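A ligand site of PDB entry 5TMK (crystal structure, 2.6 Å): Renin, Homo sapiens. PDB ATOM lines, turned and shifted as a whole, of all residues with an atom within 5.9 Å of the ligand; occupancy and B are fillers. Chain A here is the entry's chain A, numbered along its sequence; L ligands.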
ATOM      1  N   THR A  15      -2.592 -25.206  36.013  1.00  0.00           N
ATOM      2  CA  THR A  15      -1.560 -24.758  35.085  1.00  0.00           C
ATOM      3  C   THR A  15      -2.074 -23.749  34.063  1.00  0.00           C
ATOM      4  O   THR A  15      -1.334 -22.876  33.625  1.00  0.00           O
ATOM      5  CB  THR A  15      -0.870 -25.943  34.372  1.00  0.00           C
ATOM      6  OG1 THR A  15      -1.844 -26.668  33.612  1.00  0.00           O
ATOM      7  CG2 THR A  15      -0.187 -26.887  35.365  1.00  0.00           C
ATOM      8  N   GLN A  16      -3.344 -23.875  33.678  1.00  0.00           N
ATOM      9  CA  GLN A  16      -3.945 -22.957  32.708  1.00  0.00           C
ATOM     10  C   GLN A  16      -5.221 -22.326  33.241  1.00  0.00           C
ATOM     11  O   GLN A  16      -6.138 -23.035  33.673  1.00  0.00           O
ATOM     12  CB  GLN A  16      -4.254 -23.685  31.398  1.00  0.00           C
ATOM     13  CG  GLN A  16      -3.100 -24.444  30.774  1.00  0.00           C
ATOM     14  CD  GLN A  16      -3.520 -25.154  29.524  1.00  0.00           C
ATOM     15  OE1 GLN A  16      -4.156 -24.563  28.650  1.00  0.00           O
ATOM     16  NE2 GLN A  16      -3.170 -26.441  29.415  1.00  0.00           N
ATOM     17  N   TYR A  17      -5.272 -20.999  33.197  1.00  0.00           N
ATOM     18  CA  TYR A  17      -6.456 -20.221  33.563  1.00  0.00           C
ATOM     19  C   TYR A  17      -6.870 -19.386  32.388  1.00  0.00           C
ATOM     20  O   TYR A  17      -6.053 -18.629  31.833  1.00  0.00           O
ATOM     21  CB  TYR A  17      -6.171 -19.317  34.770  1.00  0.00           C
ATOM     22  CG  TYR A  17      -5.938 -20.068  36.052  1.00  0.00           C
ATOM     23  CD1 TYR A  17      -4.686 -20.628  36.349  1.00  0.00           C
ATOM     24  CD2 TYR A  17      -6.978 -20.226  36.985  1.00  0.00           C
ATOM     25  CE1 TYR A  17      -4.470 -21.322  37.527  1.00  0.00           C
ATOM     26  CE2 TYR A  17      -6.761 -20.916  38.173  1.00  0.00           C
ATOM     27  CZ  TYR A  17      -5.513 -21.462  38.444  1.00  0.00           C
ATOM     28  OH  TYR A  17      -5.300 -22.137  39.605  1.00  0.00           O
ATOM     29  N   TYR A  18      -8.139 -19.505  32.022  1.00  0.00           N
ATOM     30  CA  TYR A  18      -8.650 -18.853  30.816  1.00  0.00           C
ATOM     31  C   TYR A  18     -10.143 -18.595  30.917  1.00  0.00           C
ATOM     32  O   TYR A  18     -10.864 -19.351  31.557  1.00  0.00           O
ATOM     33  CB  TYR A  18      -8.322 -19.690  29.561  1.00  0.00           C
ATOM     34  CG  TYR A  18      -8.790 -21.115  29.631  1.00  0.00           C
ATOM     35  CD1 TYR A  18     -10.095 -21.466  29.223  1.00  0.00           C
ATOM     36  CD2 TYR A  18      -7.953 -22.127  30.109  1.00  0.00           C
ATOM     37  CE1 TYR A  18     -10.533 -22.771  29.301  1.00  0.00           C
ATOM     38  CE2 TYR A  18      -8.387 -23.444  30.180  1.00  0.00           C
ATOM     39  CZ  TYR A  18      -9.675 -23.758  29.779  1.00  0.00           C
ATOM     40  OH  TYR A  18     -10.115 -25.067  29.847  1.00  0.00           O
ATOM     41  N   VAL A  33      -6.313 -16.661  27.615  1.00  0.00           N
ATOM     42  CA  VAL A  33      -5.544 -16.330  28.801  1.00  0.00           C
ATOM     43  C   VAL A  33      -5.495 -14.813  28.893  1.00  0.00           C
ATOM     44  O   VAL A  33      -5.207 -14.129  27.909  1.00  0.00           O
ATOM     45  CB  VAL A  33      -4.107 -16.906  28.743  1.00  0.00           C
ATOM     46  CG1 VAL A  33      -3.245 -16.372  29.869  1.00  0.00           C
ATOM     47  CG2 VAL A  33      -4.145 -18.417  28.818  1.00  0.00           C
ATOM     48  N   ASP A  35      -3.437 -11.945  30.278  1.00  0.00           N
ATOM     49  CA  ASP A  35      -2.000 -11.958  30.522  1.00  0.00           C
ATOM     50  C   ASP A  35      -1.403 -10.571  30.803  1.00  0.00           C
ATOM     51  O   ASP A  35      -1.209  -9.771  29.885  1.00  0.00           O
ATOM     52  CB  ASP A  35      -1.281 -12.664  29.351  1.00  0.00           C
ATOM     53  CG  ASP A  35       0.235 -12.585  29.438  1.00  0.00           C
ATOM     54  OD1 ASP A  35       0.793 -12.570  30.555  1.00  0.00           O
ATOM     55  OD2 ASP A  35       0.886 -12.545  28.374  1.00  0.00           O
ATOM     56  N   THR A  36      -1.089 -10.319  32.066  1.00  0.00           N
ATOM     57  CA  THR A  36      -0.428  -9.067  32.462  1.00  0.00           C
ATOM     58  C   THR A  36       1.030  -8.966  31.972  1.00  0.00           C
ATOM     59  O   THR A  36       1.626  -7.887  32.031  1.00  0.00           O
ATOM     60  CB  THR A  36      -0.481  -8.845  33.987  1.00  0.00           C
ATOM     61  OG1 THR A  36      -0.009 -10.026  34.670  1.00  0.00           O
ATOM     62  CG2 THR A  36      -1.905  -8.542  34.438  1.00  0.00           C
ATOM     63  N   GLY A  37       1.583 -10.077  31.493  1.00  0.00           N
ATOM     64  CA  GLY A  37       2.956 -10.141  31.006  1.00  0.00           C
ATOM     65  C   GLY A  37       3.126  -9.804  29.539  1.00  0.00           C
ATOM     66  O   GLY A  37       4.246  -9.829  29.034  1.00  0.00           O
ATOM     67  N   SER A  38       2.025  -9.487  28.854  1.00  0.00           N
ATOM     68  CA  SER A  38       2.060  -8.996  27.464  1.00  0.00           C
ATOM     69  C   SER A  38       0.884  -8.045  27.203  1.00  0.00           C
ATOM     70  O   SER A  38       0.040  -7.847  28.076  1.00  0.00           O
ATOM     71  CB  SER A  38       2.066 -10.155  26.463  1.00  0.00           C
ATOM     72  OG  SER A  38       0.829 -10.855  26.489  1.00  0.00           O
ATOM     73  N   TRP A  42      -4.573 -11.801  20.626  1.00  0.00           N
ATOM     74  CA  TRP A  42      -4.566 -12.677  19.452  1.00  0.00           C
ATOM     75  C   TRP A  42      -5.415 -13.911  19.644  1.00  0.00           C
ATOM     76  O   TRP A  42      -5.548 -14.422  20.753  1.00  0.00           O
ATOM     77  CB  TRP A  42      -3.149 -13.070  19.044  1.00  0.00           C
ATOM     78  CG  TRP A  42      -2.424 -13.984  20.000  1.00  0.00           C
ATOM     79  CD1 TRP A  42      -1.604 -13.610  21.005  1.00  0.00           C
ATOM     80  CD2 TRP A  42      -2.446 -15.428  20.018  1.00  0.00           C
ATOM     81  NE1 TRP A  42      -1.092 -14.715  21.646  1.00  0.00           N
ATOM     82  CE2 TRP A  42      -1.603 -15.848  21.065  1.00  0.00           C
ATOM     83  CE3 TRP A  42      -3.099 -16.412  19.250  1.00  0.00           C
ATOM     84  CZ2 TRP A  42      -1.386 -17.200  21.377  1.00  0.00           C
ATOM     85  CZ3 TRP A  42      -2.879 -17.754  19.547  1.00  0.00           C
ATOM     86  CH2 TRP A  42      -2.027 -18.139  20.613  1.00  0.00           C
ATOM     87  N   ARG A  79       6.782 -12.774  20.081  1.00  0.00           N
ATOM     88  CA  ARG A  79       7.768 -13.692  20.638  1.00  0.00           C
ATOM     89  C   ARG A  79       7.616 -13.723  22.146  1.00  0.00           C
ATOM     90  O   ARG A  79       8.025 -12.807  22.846  1.00  0.00           O
ATOM     91  CB  ARG A  79       9.190 -13.300  20.221  1.00  0.00           C
ATOM     92  N   TYR A  80       6.990 -14.789  22.639  1.00  0.00           N
ATOM     93  CA  TYR A  80       6.942 -15.070  24.063  1.00  0.00           C
ATOM     94  C   TYR A  80       8.202 -15.841  24.465  1.00  0.00           C
ATOM     95  O   TYR A  80       8.920 -16.341  23.594  1.00  0.00           O
ATOM     96  CB  TYR A  80       5.686 -15.847  24.427  1.00  0.00           C
ATOM     97  CG  TYR A  80       4.389 -15.139  24.062  1.00  0.00           C
ATOM     98  CD1 TYR A  80       3.911 -14.071  24.826  1.00  0.00           C
ATOM     99  CD2 TYR A  80       3.628 -15.564  22.961  1.00  0.00           C
ATOM    100  CE1 TYR A  80       2.724 -13.427  24.504  1.00  0.00           C
ATOM    101  CE2 TYR A  80       2.431 -14.927  22.632  1.00  0.00           C
ATOM    102  CZ  TYR A  80       1.987 -13.871  23.407  1.00  0.00           C
ATOM    103  OH  TYR A  80       0.809 -13.247  23.080  1.00  0.00           O
ATOM    104  N   SER A  81       8.466 -15.941  25.770  1.00  0.00           N
ATOM    105  CA  SER A  81       9.609 -16.692  26.294  1.00  0.00           C
ATOM    106  C   SER A  81       9.618 -18.148  25.845  1.00  0.00           C
ATOM    107  O   SER A  81      10.681 -18.759  25.743  1.00  0.00           O
ATOM    108  CB  SER A  81       9.640 -16.693  27.836  1.00  0.00           C
ATOM    109  OG  SER A  81       8.845 -15.686  28.420  1.00  0.00           O
ATOM    110  N   THR A  82       8.430 -18.688  25.586  1.00  0.00           N
ATOM    111  CA  THR A  82       8.241 -20.141  25.391  1.00  0.00           C
ATOM    112  C   THR A  82       7.733 -20.518  24.001  1.00  0.00           C
ATOM    113  O   THR A  82       7.437 -21.690  23.741  1.00  0.00           O
ATOM    114  CB  THR A  82       7.298 -20.709  26.468  1.00  0.00           C
ATOM    115  OG1 THR A  82       6.209 -19.802  26.683  1.00  0.00           O
ATOM    116  CG2 THR A  82       8.043 -20.931  27.797  1.00  0.00           C
ATOM    117  N   PRO A 115       4.104 -24.583  22.299  1.00  0.00           N
ATOM    118  CA  PRO A 115       3.352 -25.295  23.342  1.00  0.00           C
ATOM    119  C   PRO A 115       1.835 -25.397  23.093  1.00  0.00           C
ATOM    120  O   PRO A 115       1.105 -25.886  23.960  1.00  0.00           O
ATOM    121  CB  PRO A 115       3.585 -24.395  24.568  1.00  0.00           C
ATOM    122  CG  PRO A 115       3.587 -23.015  23.978  1.00  0.00           C
ATOM    123  CD  PRO A 115       4.193 -23.132  22.591  1.00  0.00           C
ATOM    124  N   PHE A 116       1.362 -24.949  21.943  1.00  0.00           N
ATOM    125  CA  PHE A 116      -0.069 -24.679  21.767  1.00  0.00           C
ATOM    126  C   PHE A 116      -0.984 -25.890  21.587  1.00  0.00           C
ATOM    127  O   PHE A 116      -2.175 -25.805  21.855  1.00  0.00           O
ATOM    128  CB  PHE A 116      -0.319 -23.574  20.736  1.00  0.00           C
ATOM    129  CG  PHE A 116       0.264 -22.258  21.150  1.00  0.00           C
ATOM    130  CD1 PHE A 116      -0.313 -21.523  22.179  1.00  0.00           C
ATOM    131  CD2 PHE A 116       1.434 -21.778  20.537  1.00  0.00           C
ATOM    132  CE1 PHE A 116       0.248 -20.322  22.583  1.00  0.00           C
ATOM    133  CE2 PHE A 116       2.000 -20.585  20.943  1.00  0.00           C
ATOM    134  CZ  PHE A 116       1.403 -19.842  21.961  1.00  0.00           C
ATOM    135  N   LEU A 118      -0.808 -28.140  23.644  1.00  0.00           N
ATOM    136  CA  LEU A 118      -1.023 -28.476  25.042  1.00  0.00           C
ATOM    137  C   LEU A 118      -1.918 -27.440  25.744  1.00  0.00           C
ATOM    138  O   LEU A 118      -2.201 -27.559  26.934  1.00  0.00           O
ATOM    139  CB  LEU A 118       0.310 -28.654  25.771  1.00  0.00           C
ATOM    140  CG  LEU A 118       1.221 -29.785  25.260  1.00  0.00           C
ATOM    141  CD1 LEU A 118       2.669 -29.531  25.644  1.00  0.00           C
ATOM    142  CD2 LEU A 118       0.781 -31.161  25.746  1.00  0.00           C
ATOM    143  N   ALA A 119      -2.358 -26.447  24.974  1.00  0.00           N
ATOM    144  CA  ALA A 119      -3.191 -25.352  25.479  1.00  0.00           C
ATOM    145  C   ALA A 119      -4.671 -25.670  25.376  1.00  0.00           C
ATOM    146  O   ALA A 119      -5.175 -26.086  24.319  1.00  0.00           O
ATOM    147  CB  ALA A 119      -2.875 -24.072  24.720  1.00  0.00           C
ATOM    148  N   GLU A 120      -5.381 -25.479  26.482  1.00  0.00           N
ATOM    149  CA  GLU A 120      -6.833 -25.518  26.481  1.00  0.00           C
ATOM    150  C   GLU A 120      -7.427 -24.195  25.974  1.00  0.00           C
ATOM    151  O   GLU A 120      -8.546 -24.171  25.468  1.00  0.00           O
ATOM    152  CB  GLU A 120      -7.375 -25.877  27.857  1.00  0.00           C
ATOM    153  CG  GLU A 120      -7.470 -27.368  28.134  1.00  0.00           C
ATOM    154  CD  GLU A 120      -8.575 -28.061  27.355  1.00  0.00           C
ATOM    155  OE1 GLU A 120      -9.547 -27.389  26.936  1.00  0.00           O
ATOM    156  OE2 GLU A 120      -8.462 -29.293  27.157  1.00  0.00           O
ATOM    157  N   PHE A 121      -6.674 -23.109  26.131  1.00  0.00           N
ATOM    158  CA  PHE A 121      -7.052 -21.799  25.606  1.00  0.00           C
ATOM    159  C   PHE A 121      -6.725 -21.711  24.113  1.00  0.00           C
ATOM    160  O   PHE A 121      -5.832 -22.418  23.626  1.00  0.00           O
ATOM    161  CB  PHE A 121      -6.343 -20.678  26.384  1.00  0.00           C
ATOM    162  CG  PHE A 121      -4.830 -20.744  26.351  1.00  0.00           C
ATOM    163  CD1 PHE A 121      -4.126 -21.536  27.267  1.00  0.00           C
ATOM    164  CD2 PHE A 121      -4.105 -19.979  25.431  1.00  0.00           C
ATOM    165  CE1 PHE A 121      -2.725 -21.585  27.251  1.00  0.00           C
ATOM    166  CE2 PHE A 121      -2.705 -20.030  25.406  1.00  0.00           C
ATOM    167  CZ  PHE A 121      -2.019 -20.836  26.317  1.00  0.00           C
ATOM    168  N   VAL A 124      -4.777 -15.245  23.547  1.00  0.00           N
ATOM    169  CA  VAL A 124      -4.302 -14.447  24.676  1.00  0.00           C
ATOM    170  C   VAL A 124      -4.918 -13.048  24.624  1.00  0.00           C
ATOM    171  O   VAL A 124      -5.038 -12.447  23.553  1.00  0.00           O
ATOM    172  CB  VAL A 124      -2.754 -14.318  24.689  1.00  0.00           C
ATOM    173  CG1 VAL A 124      -2.264 -13.527  25.892  1.00  0.00           C
ATOM    174  CG2 VAL A 124      -2.080 -15.684  24.679  1.00  0.00           C
ATOM    175  N   GLN A 132       4.682  -2.071  25.791  1.00  0.00           N
ATOM    176  CA  GLN A 132       5.166  -3.419  25.498  1.00  0.00           C
ATOM    177  C   GLN A 132       4.354  -4.134  24.397  1.00  0.00           C
ATOM    178  O   GLN A 132       4.654  -5.277  24.041  1.00  0.00           O
ATOM    179  CB  GLN A 132       5.279  -4.271  26.785  1.00  0.00           C
ATOM    180  CG  GLN A 132       4.181  -4.023  27.817  1.00  0.00           C
ATOM    181  CD  GLN A 132       4.138  -5.026  28.971  1.00  0.00           C
ATOM    182  OE1 GLN A 132       4.667  -6.147  28.860  1.00  0.00           O
ATOM    183  NE2 GLN A 132       3.493  -4.634  30.075  1.00  0.00           N
ATOM    184  N   TYR A 159      -7.387 -16.452  41.160  1.00  0.00           N
ATOM    185  CA  TYR A 159      -7.158 -17.809  40.642  1.00  0.00           C
ATOM    186  C   TYR A 159      -7.429 -18.819  41.738  1.00  0.00           C
ATOM    187  O   TYR A 159      -6.767 -18.820  42.775  1.00  0.00           O
ATOM    188  CB  TYR A 159      -5.711 -17.988  40.145  1.00  0.00           C
ATOM    189  CG  TYR A 159      -5.398 -17.379  38.791  1.00  0.00           C
ATOM    190  CD1 TYR A 159      -6.395 -16.836  37.972  1.00  0.00           C
ATOM    191  CD2 TYR A 159      -4.087 -17.373  38.307  1.00  0.00           C
ATOM    192  CE1 TYR A 159      -6.086 -16.284  36.734  1.00  0.00           C
ATOM    193  CE2 TYR A 159      -3.774 -16.829  37.071  1.00  0.00           C
ATOM    194  CZ  TYR A 159      -4.779 -16.293  36.289  1.00  0.00           C
ATOM    195  OH  TYR A 159      -4.481 -15.755  35.067  1.00  0.00           O
ATOM    196  N   LEU A 221       8.326  -9.677  37.937  1.00  0.00           N
ATOM    197  CA  LEU A 221       7.220  -9.451  37.028  1.00  0.00           C
ATOM    198  C   LEU A 221       5.997 -10.196  37.558  1.00  0.00           C
ATOM    199  O   LEU A 221       6.087 -11.362  37.914  1.00  0.00           O
ATOM    200  CB  LEU A 221       7.578  -9.950  35.641  1.00  0.00           C
ATOM    201  CG  LEU A 221       6.604  -9.614  34.510  1.00  0.00           C
ATOM    202  CD1 LEU A 221       7.070  -8.378  33.772  1.00  0.00           C
ATOM    203  CD2 LEU A 221       6.502 -10.801  33.574  1.00  0.00           C
ATOM    204  N   ASP A 223       2.909 -11.834  36.439  1.00  0.00           N
ATOM    205  CA  ASP A 223       2.527 -12.386  35.140  1.00  0.00           C
ATOM    206  C   ASP A 223       1.357 -13.383  35.262  1.00  0.00           C
ATOM    207  O   ASP A 223       1.558 -14.585  35.449  1.00  0.00           O
ATOM    208  CB  ASP A 223       3.751 -13.067  34.502  1.00  0.00           C
ATOM    209  CG  ASP A 223       3.548 -13.476  33.037  1.00  0.00           C
ATOM    210  OD1 ASP A 223       2.416 -13.356  32.509  1.00  0.00           O
ATOM    211  OD2 ASP A 223       4.537 -13.930  32.398  1.00  0.00           O
ATOM    212  N   THR A 224       0.143 -12.861  35.135  1.00  0.00           N
ATOM    213  CA  THR A 224      -1.083 -13.669  35.230  1.00  0.00           C
ATOM    214  C   THR A 224      -1.197 -14.717  34.118  1.00  0.00           C
ATOM    215  O   THR A 224      -1.988 -15.653  34.232  1.00  0.00           O
ATOM    216  CB  THR A 224      -2.343 -12.780  35.160  1.00  0.00           C
ATOM    217  OG1 THR A 224      -2.376 -12.075  33.905  1.00  0.00           O
ATOM    218  CG2 THR A 224      -2.411 -11.799  36.325  1.00  0.00           C
ATOM    219  N   GLY A 225      -0.404 -14.547  33.058  1.00  0.00           N
ATOM    220  CA  GLY A 225      -0.446 -15.415  31.897  1.00  0.00           C
ATOM    221  C   GLY A 225       0.513 -16.579  31.989  1.00  0.00           C
ATOM    222  O   GLY A 225       0.613 -17.366  31.050  1.00  0.00           O
ATOM    223  N   ALA A 226       1.208 -16.690  33.125  1.00  0.00           N
ATOM    224  CA  ALA A 226       2.188 -17.755  33.350  1.00  0.00           C
ATOM    225  C   ALA A 226       1.692 -18.723  34.413  1.00  0.00           C
ATOM    226  O   ALA A 226       1.003 -18.318  35.357  1.00  0.00           O
ATOM    227  CB  ALA A 226       3.525 -17.154  33.742  1.00  0.00           C
ATOM    228  N   SER A 227       2.052 -19.995  34.245  1.00  0.00           N
ATOM    229  CA  SER A 227       1.617 -21.055  35.142  1.00  0.00           C
ATOM    230  C   SER A 227       2.379 -20.999  36.457  1.00  0.00           C
ATOM    231  O   SER A 227       1.793 -21.100  37.545  1.00  0.00           O
ATOM    232  CB  SER A 227       1.864 -22.421  34.508  1.00  0.00           C
ATOM    233  OG  SER A 227       1.247 -22.540  33.242  1.00  0.00           O
ATOM    234  N   MET A 300      13.017 -19.410  33.559  1.00  0.00           N
ATOM    235  CA  MET A 300      12.706 -18.656  32.338  1.00  0.00           C
ATOM    236  C   MET A 300      13.681 -17.504  32.213  1.00  0.00           C
ATOM    237  O   MET A 300      13.741 -16.624  33.070  1.00  0.00           O
ATOM    238  CB  MET A 300      11.271 -18.122  32.326  1.00  0.00           C
ATOM    239  CG  MET A 300      10.205 -19.130  31.951  1.00  0.00           C
ATOM    240  SD  MET A 300       8.842 -18.408  31.003  1.00  0.00           S
ATOM    241  CE  MET A 300       8.036 -17.316  32.176  1.00  0.00           C
ATOM    242  N   ILE A 302      14.559 -14.243  30.615  1.00  0.00           N
ATOM    243  CA  ILE A 302      13.915 -13.112  29.979  1.00  0.00           C
ATOM    244  C   ILE A 302      15.003 -12.077  29.660  1.00  0.00           C
ATOM    245  O   ILE A 302      15.727 -11.669  30.569  1.00  0.00           O
ATOM    246  CB  ILE A 302      12.778 -12.539  30.859  1.00  0.00           C
ATOM    247  CG1 ILE A 302      11.647 -13.584  30.983  1.00  0.00           C
ATOM    248  CG2 ILE A 302      12.230 -11.232  30.279  1.00  0.00           C
ATOM    249  CD1 ILE A 302      10.940 -13.607  32.324  1.00  0.00           C
ATOM    250  N   PRO A 303      15.144 -11.696  28.372  1.00  0.00           N
ATOM    251  CA  PRO A 303      16.180 -10.745  27.960  1.00  0.00           C
ATOM    252  C   PRO A 303      15.839  -9.303  28.344  1.00  0.00           C
ATOM    253  O   PRO A 303      14.670  -9.014  28.634  1.00  0.00           O
ATOM    254  CB  PRO A 303      16.211 -10.907  26.437  1.00  0.00           C
ATOM    255  CG  PRO A 303      14.831 -11.332  26.074  1.00  0.00           C
ATOM    256  CD  PRO A 303      14.357 -12.191  27.213  1.00  0.00           C
ATOM    257  N   THR A 306      13.133  -6.049  29.794  1.00  0.00           N
ATOM    258  CA  THR A 306      12.234  -6.643  30.812  1.00  0.00           C
ATOM    259  C   THR A 306      13.023  -7.455  31.853  1.00  0.00           C
ATOM    260  O   THR A 306      12.802  -7.298  33.057  1.00  0.00           O
ATOM    261  CB  THR A 306      11.107  -7.494  30.176  1.00  0.00           C
ATOM    262  OG1 THR A 306      10.434  -6.717  29.177  1.00  0.00           O
ATOM    263  CG2 THR A 306      10.074  -7.924  31.214  1.00  0.00           C
ATOM    264  N   THR A 309      14.611 -11.226  35.133  1.00  0.00           N
ATOM    265  CA  THR A 309      13.536 -10.994  36.094  1.00  0.00           C
ATOM    266  C   THR A 309      12.872 -12.301  36.559  1.00  0.00           C
ATOM    267  O   THR A 309      12.803 -13.281  35.802  1.00  0.00           O
ATOM    268  CB  THR A 309      12.457 -10.012  35.546  1.00  0.00           C
ATOM    269  OG1 THR A 309      11.472  -9.746  36.549  1.00  0.00           O
ATOM    270  CG2 THR A 309      11.749 -10.533  34.281  1.00  0.00           C
ATOM    271  N   ALA A 314       0.661 -18.104  38.140  1.00  0.00           N
ATOM    272  CA  ALA A 314      -0.512 -18.688  38.822  1.00  0.00           C
ATOM    273  C   ALA A 314      -0.195 -19.256  40.212  1.00  0.00           C
ATOM    274  O   ALA A 314      -1.004 -19.098  41.126  1.00  0.00           O
ATOM    275  CB  ALA A 314      -1.188 -19.729  37.949  1.00  0.00           C
HETATM  276  C1  LIG L   1      -1.278 -20.730  31.046  1.00  0.00           C
HETATM  277  C2  LIG L   1      -0.305 -20.362  29.929  1.00  0.00           C
HETATM  278  C3  LIG L   1       1.132 -20.710  30.334  1.00  0.00           C
HETATM  279  C4  LIG L   1       2.795 -19.942  28.556  1.00  0.00           C
HETATM  280  C5  LIG L   1       2.802 -21.744  27.227  1.00  0.00           C
HETATM  281  C6  LIG L   1       0.531 -23.798  27.273  1.00  0.00           C
HETATM  282  C7  LIG L   1      -0.133 -25.676  28.630  1.00  0.00           C
HETATM  283  C8  LIG L   1       1.198 -23.945  29.617  1.00  0.00           C
HETATM  284  C9  LIG L   1       2.802 -17.369  26.962  1.00  0.00           C
HETATM  285  C10 LIG L   1       1.328 -17.142  26.561  1.00  0.00           C
HETATM  286  C11 LIG L   1       0.262 -17.413  27.632  1.00  0.00           C
HETATM  287  C12 LIG L   1      -2.570 -18.821  33.817  1.00  0.00           C
HETATM  288  O1  LIG L   1      -2.706 -19.750  32.741  1.00  0.00           O
HETATM  289  C13 LIG L   1      -1.888 -19.447  31.620  1.00  0.00           C
HETATM  290  N1  LIG L   1       1.938 -20.885  29.106  1.00  0.00           N
HETATM  291  C14 LIG L   1       3.350 -20.491  27.411  1.00  0.00           C
HETATM  292  C15 LIG L   1       1.934 -21.982  28.265  1.00  0.00           C
HETATM  293  C16 LIG L   1       1.192 -23.249  28.395  1.00  0.00           C
HETATM  294  C17 LIG L   1      -0.136 -25.002  27.415  1.00  0.00           C
HETATM  295  C18 LIG L   1       0.523 -25.147  29.738  1.00  0.00           C
HETATM  296  C19 LIG L   1       3.185 -18.618  29.094  1.00  0.00           C
HETATM  297  O2  LIG L   1       3.541 -18.625  30.251  1.00  0.00           O
HETATM  298  N2  LIG L   1       3.199 -17.444  28.394  1.00  0.00           N
HETATM  299  C20 LIG L   1       1.019 -17.962  25.316  1.00  0.00           C
HETATM  300  C21 LIG L   1       3.686 -16.245  29.136  1.00  0.00           C
HETATM  301  C22 LIG L   1       2.592 -15.182  29.392  1.00  0.00           C
HETATM  302  N3  LIG L   1       3.131 -13.898  29.875  1.00  0.00           N
HETATM  303  C23 LIG L   1       4.152 -13.323  28.989  1.00  0.00           C
HETATM  304  C24 LIG L   1       5.370 -14.260  28.985  1.00  0.00           C
HETATM  305  C25 LIG L   1       4.961 -15.661  28.476  1.00  0.00           C
HETATM  306  C26 LIG L   1       6.491 -13.667  28.146  1.00  0.00           C
HETATM  307  O3  LIG L   1       6.477 -13.890  26.948  1.00  0.00           O
HETATM  308  N4  LIG L   1       7.498 -12.908  28.646  1.00  0.00           N
HETATM  309  C27 LIG L   1       7.621 -12.559  30.086  1.00  0.00           C
HETATM  310  C28 LIG L   1       7.668 -11.021  30.171  1.00  0.00           C
HETATM  311  O4  LIG L   1       8.716 -10.517  29.318  1.00  0.00           O
HETATM  312  C29 LIG L   1       8.596 -10.829  27.917  1.00  0.00           C
HETATM  313  C30 LIG L   1       8.546 -12.367  27.748  1.00  0.00           C
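OG of Ser 81 lies close to O3 of the ligand (3.3 Å). OD1 of Asp 223 lies within salt-bridge range of N3 of the ligand (2.8 Å). The backbone NH of Ser 81 lies within hydrogen-bond range of an oxygen (O3) of the ligand, at 3.1 Å. An oxygen (O1) of the ligand sits at hydrogen-bond distance from the backbone NH of Tyr 17 (2.9 Å). The side-chain carboxylate (OD1) of Asp 35 lies within salt-bridge range of a nitrogen (N3) of the ligand (2.8 Å).
The side-chain carboxylate of Asp 35 sits close to the backbone NH of Gly 225 (3.4 Å). The backbone NH of Gly 37 sits at hydrogen-bond distance from the side-chain carboxylate of Asp 35, at 2.8 Å. OG of Ser 38 is in hydrogen-bond range of OD2 of Asp 35 (2.5 Å). O of Thr 15 lies within hydrogen-bond range of OG of Ser 227, at 2.6 Å. The backbone carbonyl oxygen (O) of Ala 226 is in hydrogen-bond range of the backbone NH (N) of Ala 314 (2.8 Å). The side-chain carboxylate (OD1) of Asp 223 sits close to the side-chain carboxylate (OD1) of Asp 35, 2.7 Å away. The backbone NH (N) of Val 124 is in hydrogen-bond range of the backbone carbonyl oxygen (O) of Trp 42 (3.0 Å). OG of Ser 81 sits close to SD of Met 300 (3.8 Å).
The backbone carbonyl oxygen (O) of Gly 225 sits close to an oxygen (O2) of the ligand (3.3 Å). Thr 15 touches the ligand. NE2 of Gln 16 touches C7 of the ligand, at 3.2 Å. CG2 of Val 33 touches C13 of the ligand, at 3.7 Å. Gly 37 touches the ligand. Tyr 80 touches the ligand (CA to O3, 3.2 Å). Thr 82 touches the ligand. Pro 115 touches the ligand. Phe 116 touches the ligand. O of Leu 118 touches C7 of the ligand, 3.3 Å away. Ala 119 touches the ligand (N to C17, 3.6 Å). CE1 of Phe 121 touches C2 of the ligand, 3.8 Å away. CG2 of Val 124 touches C20 of the ligand, at 3.9 Å. Tyr 159 touches the ligand. CD2 of Leu 221 touches C28 of the ligand, 3.6 Å away. O of Thr 224 touches C12 of the ligand, at 3.2 Å. CA of Ala 226 touches O2 of the ligand (3.5 Å). OG of Ser 227 touches C3 of the ligand, 3.4 Å away. Ile 302 touches the ligand. CG2 of Thr 306 touches O4 of the ligand, 3.5 Å away. Hydrophobic or aromatic side chains that line the ligand: Tyr 17, Val 33, Tyr 80, Pro 115, Phe 116, Ala 119, Phe 121, Val 124, Leu 221, Ala 226 and Ile 302. Within 4 Å of the ligand: Thr 15, Gln 16, Tyr 17, Val 33, Asp 35, Gly 37, Tyr 80, Ser 81, Thr 82, Pro 115, Phe 116, Leu 118, Ala 119, Phe 121, Val 124, Tyr 159, Leu 221, Asp 223, Thr 224, Gly 225, Ala 226, Ser 227, Ile 302 and Thr 306. Along chain A the residues within 4 Å of the ligand span positions 15 to 306. The nearest printed residue that does not touch the ligand is Ser 38 (4.4 Å).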
